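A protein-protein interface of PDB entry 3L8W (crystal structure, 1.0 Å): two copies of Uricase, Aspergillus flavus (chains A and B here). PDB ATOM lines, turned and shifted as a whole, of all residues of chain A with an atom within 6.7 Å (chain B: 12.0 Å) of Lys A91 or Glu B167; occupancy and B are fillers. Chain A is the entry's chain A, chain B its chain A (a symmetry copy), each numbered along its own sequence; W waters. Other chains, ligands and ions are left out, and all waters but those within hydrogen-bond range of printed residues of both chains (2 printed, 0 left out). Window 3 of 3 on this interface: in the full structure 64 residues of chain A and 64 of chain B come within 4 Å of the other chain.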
ATOM      1  N   ILE A  67      29.934   5.838   8.618  1.00  0.00           N
ATOM      2  CA  ILE A  67      29.728   4.402   8.373  1.00  0.00           C
ATOM      3  C   ILE A  67      30.031   4.041   6.927  1.00  0.00           C
ATOM      4  O   ILE A  67      30.649   3.019   6.616  1.00  0.00           O
ATOM      5  CB  ILE A  67      28.303   4.036   8.790  1.00  0.00           C
ATOM      6  CG1 ILE A  67      28.128   4.116  10.312  1.00  0.00           C
ATOM      7  CG2 ILE A  67      27.884   2.670   8.265  1.00  0.00           C
ATOM      8  CD1 ILE A  67      26.685   4.262  10.783  1.00  0.00           C
ATOM      9  N   THR A  86      23.348   7.325  -3.165  1.00  0.00           N
ATOM     10  CA  THR A  86      22.472   6.196  -3.497  1.00  0.00           C
ATOM     11  C   THR A  86      21.868   5.616  -2.219  1.00  0.00           C
ATOM     12  O   THR A  86      20.705   5.222  -2.147  1.00  0.00           O
ATOM     13  CB  THR A  86      23.245   5.141  -4.287  1.00  0.00           C
ATOM     14  OG1 THR A  86      23.541   5.719  -5.552  1.00  0.00           O
ATOM     15  CG2 THR A  86      22.383   3.897  -4.590  1.00  0.00           C
ATOM     16  N   HIS A  87      22.710   5.516  -1.148  1.00  0.00           N
ATOM     17  CA  HIS A  87      22.239   4.974   0.109  1.00  0.00           C
ATOM     18  C   HIS A  87      20.974   5.683   0.571  1.00  0.00           C
ATOM     19  O   HIS A  87      20.006   5.031   0.995  1.00  0.00           O
ATOM     20  CB  HIS A  87      23.355   5.074   1.163  1.00  0.00           C
ATOM     21  CG  HIS A  87      22.760   4.900   2.541  1.00  0.00           C
ATOM     22  ND1 HIS A  87      22.463   3.651   3.045  1.00  0.00           N
ATOM     23  CD2 HIS A  87      22.385   5.791   3.487  1.00  0.00           C
ATOM     24  CE1 HIS A  87      21.939   3.818   4.248  1.00  0.00           C
ATOM     25  NE2 HIS A  87      21.873   5.095   4.533  1.00  0.00           N
ATOM     26  N   PHE A  88      20.947   7.028   0.560  1.00  0.00           N
ATOM     27  CA  PHE A  88      19.813   7.721   1.156  1.00  0.00           C
ATOM     28  C   PHE A  88      18.511   7.487   0.359  1.00  0.00           C
ATOM     29  O   PHE A  88      17.446   7.342   0.980  1.00  0.00           O
ATOM     30  CB  PHE A  88      20.073   9.223   1.304  1.00  0.00           C
ATOM     31  CG  PHE A  88      21.118   9.488   2.426  1.00  0.00           C
ATOM     32  CD1 PHE A  88      20.731   9.414   3.764  1.00  0.00           C
ATOM     33  CD2 PHE A  88      22.423   9.783   2.082  1.00  0.00           C
ATOM     34  CE1 PHE A  88      21.689   9.650   4.752  1.00  0.00           C
ATOM     35  CE2 PHE A  88      23.366  10.008   3.080  1.00  0.00           C
ATOM     36  CZ  PHE A  88      23.004   9.932   4.397  1.00  0.00           C
ATOM     37  N   ILE A  89      18.623   7.504  -0.967  1.00  0.00           N
ATOM     38  CA  ILE A  89      17.384   7.316  -1.745  1.00  0.00           C
ATOM     39  C   ILE A  89      16.945   5.871  -1.713  1.00  0.00           C
ATOM     40  O   ILE A  89      15.744   5.630  -1.814  1.00  0.00           O
ATOM     41  CB  ILE A  89      17.543   7.837  -3.174  1.00  0.00           C
ATOM     42  CG1 ILE A  89      18.566   7.115  -4.051  1.00  0.00           C
ATOM     43  CG2 ILE A  89      17.807   9.363  -3.193  1.00  0.00           C
ATOM     44  CD1 ILE A  89      18.229   7.278  -5.546  1.00  0.00           C
ATOM     45  N   GLU A  90      17.825   4.891  -1.515  1.00  0.00           N
ATOM     46  CA  GLU A  90      17.390   3.512  -1.375  1.00  0.00           C
ATOM     47  C   GLU A  90      16.907   3.183   0.019  1.00  0.00           C
ATOM     48  O   GLU A  90      15.949   2.424   0.201  1.00  0.00           O
ATOM     49  CB  GLU A  90      18.560   2.594  -1.772  1.00  0.00           C
ATOM     50  CG  GLU A  90      18.867   2.685  -3.270  1.00  0.00           C
ATOM     51  CD  GLU A  90      19.849   1.632  -3.751  1.00  0.00           C
ATOM     52  OE1 GLU A  90      20.478   1.001  -2.842  1.00  0.00           O
ATOM     53  OE2 GLU A  90      19.927   1.495  -5.017  1.00  0.00           O
ATOM     54  N   LYS A  91      17.537   3.748   1.053  1.00  0.00           N
ATOM     55  CA  LYS A  91      17.167   3.406   2.424  1.00  0.00           C
ATOM     56  C   LYS A  91      15.830   4.012   2.825  1.00  0.00           C
ATOM     57  O   LYS A  91      15.074   3.381   3.574  1.00  0.00           O
ATOM     58  CB  LYS A  91      18.283   3.889   3.370  1.00  0.00           C
ATOM     59  CG  LYS A  91      18.019   3.603   4.848  1.00  0.00           C
ATOM     60  CD  LYS A  91      17.912   2.103   5.170  1.00  0.00           C
ATOM     61  CE  LYS A  91      17.469   1.899   6.591  1.00  0.00           C
ATOM     62  NZ  LYS A  91      17.288   0.447   6.923  1.00  0.00           N
ATOM     63  N   TYR A  92      15.514   5.236   2.391  1.00  0.00           N
ATOM     64  CA  TYR A  92      14.375   6.004   2.859  1.00  0.00           C
ATOM     65  C   TYR A  92      13.368   6.198   1.709  1.00  0.00           C
ATOM     66  O   TYR A  92      13.654   6.910   0.738  1.00  0.00           O
ATOM     67  CB  TYR A  92      14.745   7.401   3.445  1.00  0.00           C
ATOM     68  CG  TYR A  92      15.717   7.182   4.593  1.00  0.00           C
ATOM     69  CD1 TYR A  92      15.243   6.698   5.788  1.00  0.00           C
ATOM     70  CD2 TYR A  92      17.065   7.428   4.469  1.00  0.00           C
ATOM     71  CE1 TYR A  92      16.077   6.469   6.869  1.00  0.00           C
ATOM     72  CE2 TYR A  92      17.941   7.198   5.530  1.00  0.00           C
ATOM     73  CZ  TYR A  92      17.431   6.729   6.724  1.00  0.00           C
ATOM     74  OH  TYR A  92      18.259   6.462   7.782  1.00  0.00           O
ATOM     75  N   ASN A  93      12.212   5.557   1.777  1.00  0.00           N
ATOM     76  CA  ASN A  93      11.252   5.611   0.667  1.00  0.00           C
ATOM     77  C   ASN A  93      10.896   7.030   0.290  1.00  0.00           C
ATOM     78  O   ASN A  93      10.758   7.333  -0.882  1.00  0.00           O
ATOM     79  CB  ASN A  93       9.980   4.838   1.058  1.00  0.00           C
ATOM     80  CG  ASN A  93      10.150   3.359   1.117  1.00  0.00           C
ATOM     81  OD1 ASN A  93      11.218   2.774   0.928  1.00  0.00           O
ATOM     82  ND2 ASN A  93       9.096   2.611   1.405  1.00  0.00           N
ATOM     83  N   HIS A  94      10.776   7.904   1.291  1.00  0.00           N
ATOM     84  CA  HIS A  94      10.269   9.246   1.081  1.00  0.00           C
ATOM     85  C   HIS A  94      11.336  10.287   0.719  1.00  0.00           C
ATOM     86  O   HIS A  94      10.979  11.440   0.468  1.00  0.00           O
ATOM     87  CB  HIS A  94       9.480   9.750   2.309  1.00  0.00           C
ATOM     88  CG  HIS A  94      10.318  10.135   3.485  1.00  0.00           C
ATOM     89  ND1 HIS A  94      11.105   9.266   4.185  1.00  0.00           N
ATOM     90  CD2 HIS A  94      10.491  11.363   4.048  1.00  0.00           C
ATOM     91  CE1 HIS A  94      11.725   9.957   5.150  1.00  0.00           C
ATOM     92  NE2 HIS A  94      11.362  11.212   5.099  1.00  0.00           N
ATOM     93  N   PHE B 163      11.578  13.026  15.496  1.00  0.00           N
ATOM     94  CA  PHE B 163      12.258  12.745  14.225  1.00  0.00           C
ATOM     95  C   PHE B 163      12.384  11.237  14.002  1.00  0.00           C
ATOM     96  O   PHE B 163      12.265  10.430  14.927  1.00  0.00           O
ATOM     97  CB  PHE B 163      13.594  13.474  14.120  1.00  0.00           C
ATOM     98  CG  PHE B 163      14.482  13.251  15.338  1.00  0.00           C
ATOM     99  CD1 PHE B 163      14.430  14.138  16.404  1.00  0.00           C
ATOM    100  CD2 PHE B 163      15.332  12.179  15.392  1.00  0.00           C
ATOM    101  CE1 PHE B 163      15.273  13.941  17.509  1.00  0.00           C
ATOM    102  CE2 PHE B 163      16.181  11.990  16.470  1.00  0.00           C
ATOM    103  CZ  PHE B 163      16.122  12.877  17.511  1.00  0.00           C
ATOM    104  N   LEU B 164      12.687  10.847  12.780  1.00  0.00           N
ATOM    105  CA  LEU B 164      12.827   9.439  12.409  1.00  0.00           C
ATOM    106  C   LEU B 164      13.966   8.812  13.199  1.00  0.00           C
ATOM    107  O   LEU B 164      15.068   9.376  13.310  1.00  0.00           O
ATOM    108  CB  LEU B 164      13.087   9.316  10.905  1.00  0.00           C
ATOM    109  CG  LEU B 164      13.153   7.933  10.289  1.00  0.00           C
ATOM    110  CD1 LEU B 164      12.687   7.974   8.816  1.00  0.00           C
ATOM    111  CD2 LEU B 164      14.560   7.341  10.330  1.00  0.00           C
ATOM    112  N   ARG B 165      13.731   7.601  13.719  1.00  0.00           N
ATOM    113  CA  ARG B 165      14.719   6.842  14.441  1.00  0.00           C
ATOM    114  C   ARG B 165      14.886   5.460  13.813  1.00  0.00           C
ATOM    115  O   ARG B 165      13.948   4.673  13.704  1.00  0.00           O
ATOM    116  CB  ARG B 165      14.341   6.692  15.918  1.00  0.00           C
ATOM    117  CG  ARG B 165      13.964   7.964  16.636  1.00  0.00           C
ATOM    118  CD  ARG B 165      13.835   7.775  18.174  1.00  0.00           C
ATOM    119  NE  ARG B 165      15.184   7.570  18.671  1.00  0.00           N
ATOM    120  CZ  ARG B 165      16.027   8.564  18.980  1.00  0.00           C
ATOM    121  NH1 ARG B 165      15.664   9.847  18.864  1.00  0.00           N
ATOM    122  NH2 ARG B 165      17.235   8.255  19.407  1.00  0.00           N
ATOM    123  N   ASP B 166      16.093   5.100  13.412  1.00  0.00           N
ATOM    124  CA  ASP B 166      16.500   3.783  12.891  1.00  0.00           C
ATOM    125  C   ASP B 166      17.925   3.433  13.296  1.00  0.00           C
ATOM    126  O   ASP B 166      18.465   4.040  14.240  1.00  0.00           O
ATOM    127  CB  ASP B 166      16.289   3.766  11.378  1.00  0.00           C
ATOM    128  CG  ASP B 166      17.242   4.632  10.574  1.00  0.00           C
ATOM    129  OD1 ASP B 166      18.194   5.203  11.164  1.00  0.00           O
ATOM    130  OD2 ASP B 166      17.055   4.713   9.334  1.00  0.00           O
ATOM    131  N   GLU B 167      18.531   2.462  12.619  1.00  0.00           N
ATOM    132  CA  GLU B 167      19.840   1.923  13.026  1.00  0.00           C
ATOM    133  C   GLU B 167      20.978   2.907  12.766  1.00  0.00           C
ATOM    134  O   GLU B 167      22.122   2.591  13.169  1.00  0.00           O
ATOM    135  CB  GLU B 167      20.109   0.590  12.320  1.00  0.00           C
ATOM    136  CG  GLU B 167      20.295   0.571  10.822  1.00  0.00           C
ATOM    137  CD  GLU B 167      19.029   0.449   9.988  1.00  0.00           C
ATOM    138  OE1 GLU B 167      17.938   0.752  10.521  1.00  0.00           O
ATOM    139  OE2 GLU B 167      19.155   0.091   8.782  1.00  0.00           O
ATOM    140  N   TYR B 168      20.726   4.065  12.143  1.00  0.00           N
ATOM    141  CA  TYR B 168      21.733   5.107  11.978  1.00  0.00           C
ATOM    142  C   TYR B 168      21.596   6.208  13.033  1.00  0.00           C
ATOM    143  O   TYR B 168      22.411   7.158  12.989  1.00  0.00           O
ATOM    144  CB  TYR B 168      21.635   5.692  10.547  1.00  0.00           C
ATOM    145  CG  TYR B 168      21.943   4.637   9.494  1.00  0.00           C
ATOM    146  CD1 TYR B 168      23.218   4.397   9.038  1.00  0.00           C
ATOM    147  CD2 TYR B 168      20.945   3.867   8.908  1.00  0.00           C
ATOM    148  CE1 TYR B 168      23.524   3.449   8.068  1.00  0.00           C
ATOM    149  CE2 TYR B 168      21.204   2.897   7.974  1.00  0.00           C
ATOM    150  CZ  TYR B 168      22.489   2.694   7.553  1.00  0.00           C
ATOM    151  OH  TYR B 168      22.754   1.706   6.618  1.00  0.00           O
ATOM    152  N   THR B 169      20.610   6.131  13.924  1.00  0.00           N
ATOM    153  CA  THR B 169      20.252   7.241  14.796  1.00  0.00           C
ATOM    154  C   THR B 169      20.819   7.082  16.210  1.00  0.00           C
ATOM    155  O   THR B 169      20.555   6.069  16.858  1.00  0.00           O
ATOM    156  CB  THR B 169      18.724   7.374  14.947  1.00  0.00           C
ATOM    157  OG1 THR B 169      18.146   7.375  13.640  1.00  0.00           O
ATOM    158  CG2 THR B 169      18.312   8.606  15.712  1.00  0.00           C
ATOM    159  N   THR B 170      21.555   8.089  16.661  1.00  0.00           N
ATOM    160  CA  THR B 170      22.006   8.174  18.040  1.00  0.00           C
ATOM    161  C   THR B 170      21.469   9.399  18.757  1.00  0.00           C
ATOM    162  O   THR B 170      21.521   9.478  19.994  1.00  0.00           O
ATOM    163  CB  THR B 170      23.553   8.154  18.114  1.00  0.00           C
ATOM    164  OG1 THR B 170      24.054   9.183  17.265  1.00  0.00           O
ATOM    165  CG2 THR B 170      24.161   6.855  17.604  1.00  0.00           C
ATOM    166  N   LEU B 171      20.988  10.408  18.055  1.00  0.00           N
ATOM    167  CA  LEU B 171      20.603  11.675  18.674  1.00  0.00           C
ATOM    168  C   LEU B 171      19.438  11.522  19.641  1.00  0.00           C
ATOM    169  O   LEU B 171      18.382  10.964  19.322  1.00  0.00           O
ATOM    170  CB  LEU B 171      20.148  12.650  17.580  1.00  0.00           C
ATOM    171  CG  LEU B 171      19.759  14.069  18.019  1.00  0.00           C
ATOM    172  CD1 LEU B 171      20.969  14.792  18.600  1.00  0.00           C
ATOM    173  CD2 LEU B 171      19.152  14.865  16.878  1.00  0.00           C
ATOM    174  N   LYS B 172      19.584  12.051  20.854  1.00  0.00           N
ATOM    175  CA  LYS B 172      18.501  12.059  21.814  1.00  0.00           C
ATOM    176  C   LYS B 172      17.466  13.137  21.510  1.00  0.00           C
ATOM    177  O   LYS B 172      17.811  14.286  21.161  1.00  0.00           O
ATOM    178  CB  LYS B 172      19.038  12.286  23.243  1.00  0.00           C
ATOM    179  CG  LYS B 172      19.891  11.176  23.791  1.00  0.00           C
ATOM    180  CD  LYS B 172      19.502   9.788  23.416  1.00  0.00           C
ATOM    181  CE  LYS B 172      18.210   9.209  23.970  1.00  0.00           C
ATOM    182  NZ  LYS B 172      17.591   8.242  23.012  1.00  0.00           N
HETATM  183  O   HOH W   1      15.595   0.602   9.138  1.00  0.00           O
HETATM  184  O   HOH W   2      18.332   7.859  10.422  1.00  0.00           O
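OE2 of Glu B167 is in salt-bridge range of NZ of Lys A91 (2.7 Å). The side-chain hydroxyl (OH) of Tyr A92 sits at hydrogen-bond distance from the side-chain carboxylate (OD2) of Asp B166, 2.6 Å away.
The side-chain carboxylate of Asp B166 lies within hydrogen-bond range of the backbone NH of Tyr B168 (2.9 Å). The backbone NH (N) of Asp B166 is in hydrogen-bond range of the side-chain hydroxyl (OG1) of Thr B169, 3.1 Å away.
CD1 of Tyr B168 touches CD1 of Ile A67, at 3.9 Å. Tyr B168 touches His A87. OD2 of Asp B166 touches CE of Lys A91, at 3.95 Å. CD2 of Leu B164 touches CE1 of Tyr A92 (3.9 Å). Tyr B168 touches Tyr A92.
Lys A91 touches just these residues of chain B: Asp B166 (3.95 Å) and Glu B167 (2.7 Å). His A87 touches just one residue of chain B: Tyr B168 (3.3 Å). No residue of chain B comes within 4 Å of Ile A89. Of the printed residues of chain B, Ile A67 touches Tyr B168 (3.9 Å). Printed residues of chain A within 4 Å of Tyr B168: Ile A67, His A87 and Tyr A92. Of the printed residues of chain A, Asp B166 touches Lys A91 and Tyr A92. Printed residues of chain A within 4 Å of Leu B164: Tyr A92 (3.9 Å). The nearest printed residue of chain A that does not touch Asp B166 is His A87 (6.8 Å).
Of the 10 printed residues of chain A, 4 touch a printed residue of chain B. Hydrophobic or aromatic side chains of chain A that line the printed part of chain B: Ile A67, His A87 and Tyr A92. Of the 10 printed residues of chain B, 4 touch a printed residue of chain A. Hydrophobic or aromatic side chains of chain B within 4 Å of the printed part of chain A: Leu B164 and Tyr B168. Among the printed residues, 7 pairs touch across the chains. Among the printed residues, Asp or Glu carboxylates within 4 Å of a Lys or Arg side-chain nitrogen of the other chain: Lys A91 with Glu B167.
No position is printed for both chains.
Water W1 lies within hydrogen-bond range of the side-chain carboxylate (OE1) of Glu B167 (2.7 Å) and the side-chain amino group (NZ) of Lys A91 (2.8 Å). Water W2 lies within hydrogen-bond range of OD1 of Asp B166 (2.8 Å), OH of Tyr A92 (3.0 Å) and OG1 of Thr B169 (3.3 Å).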
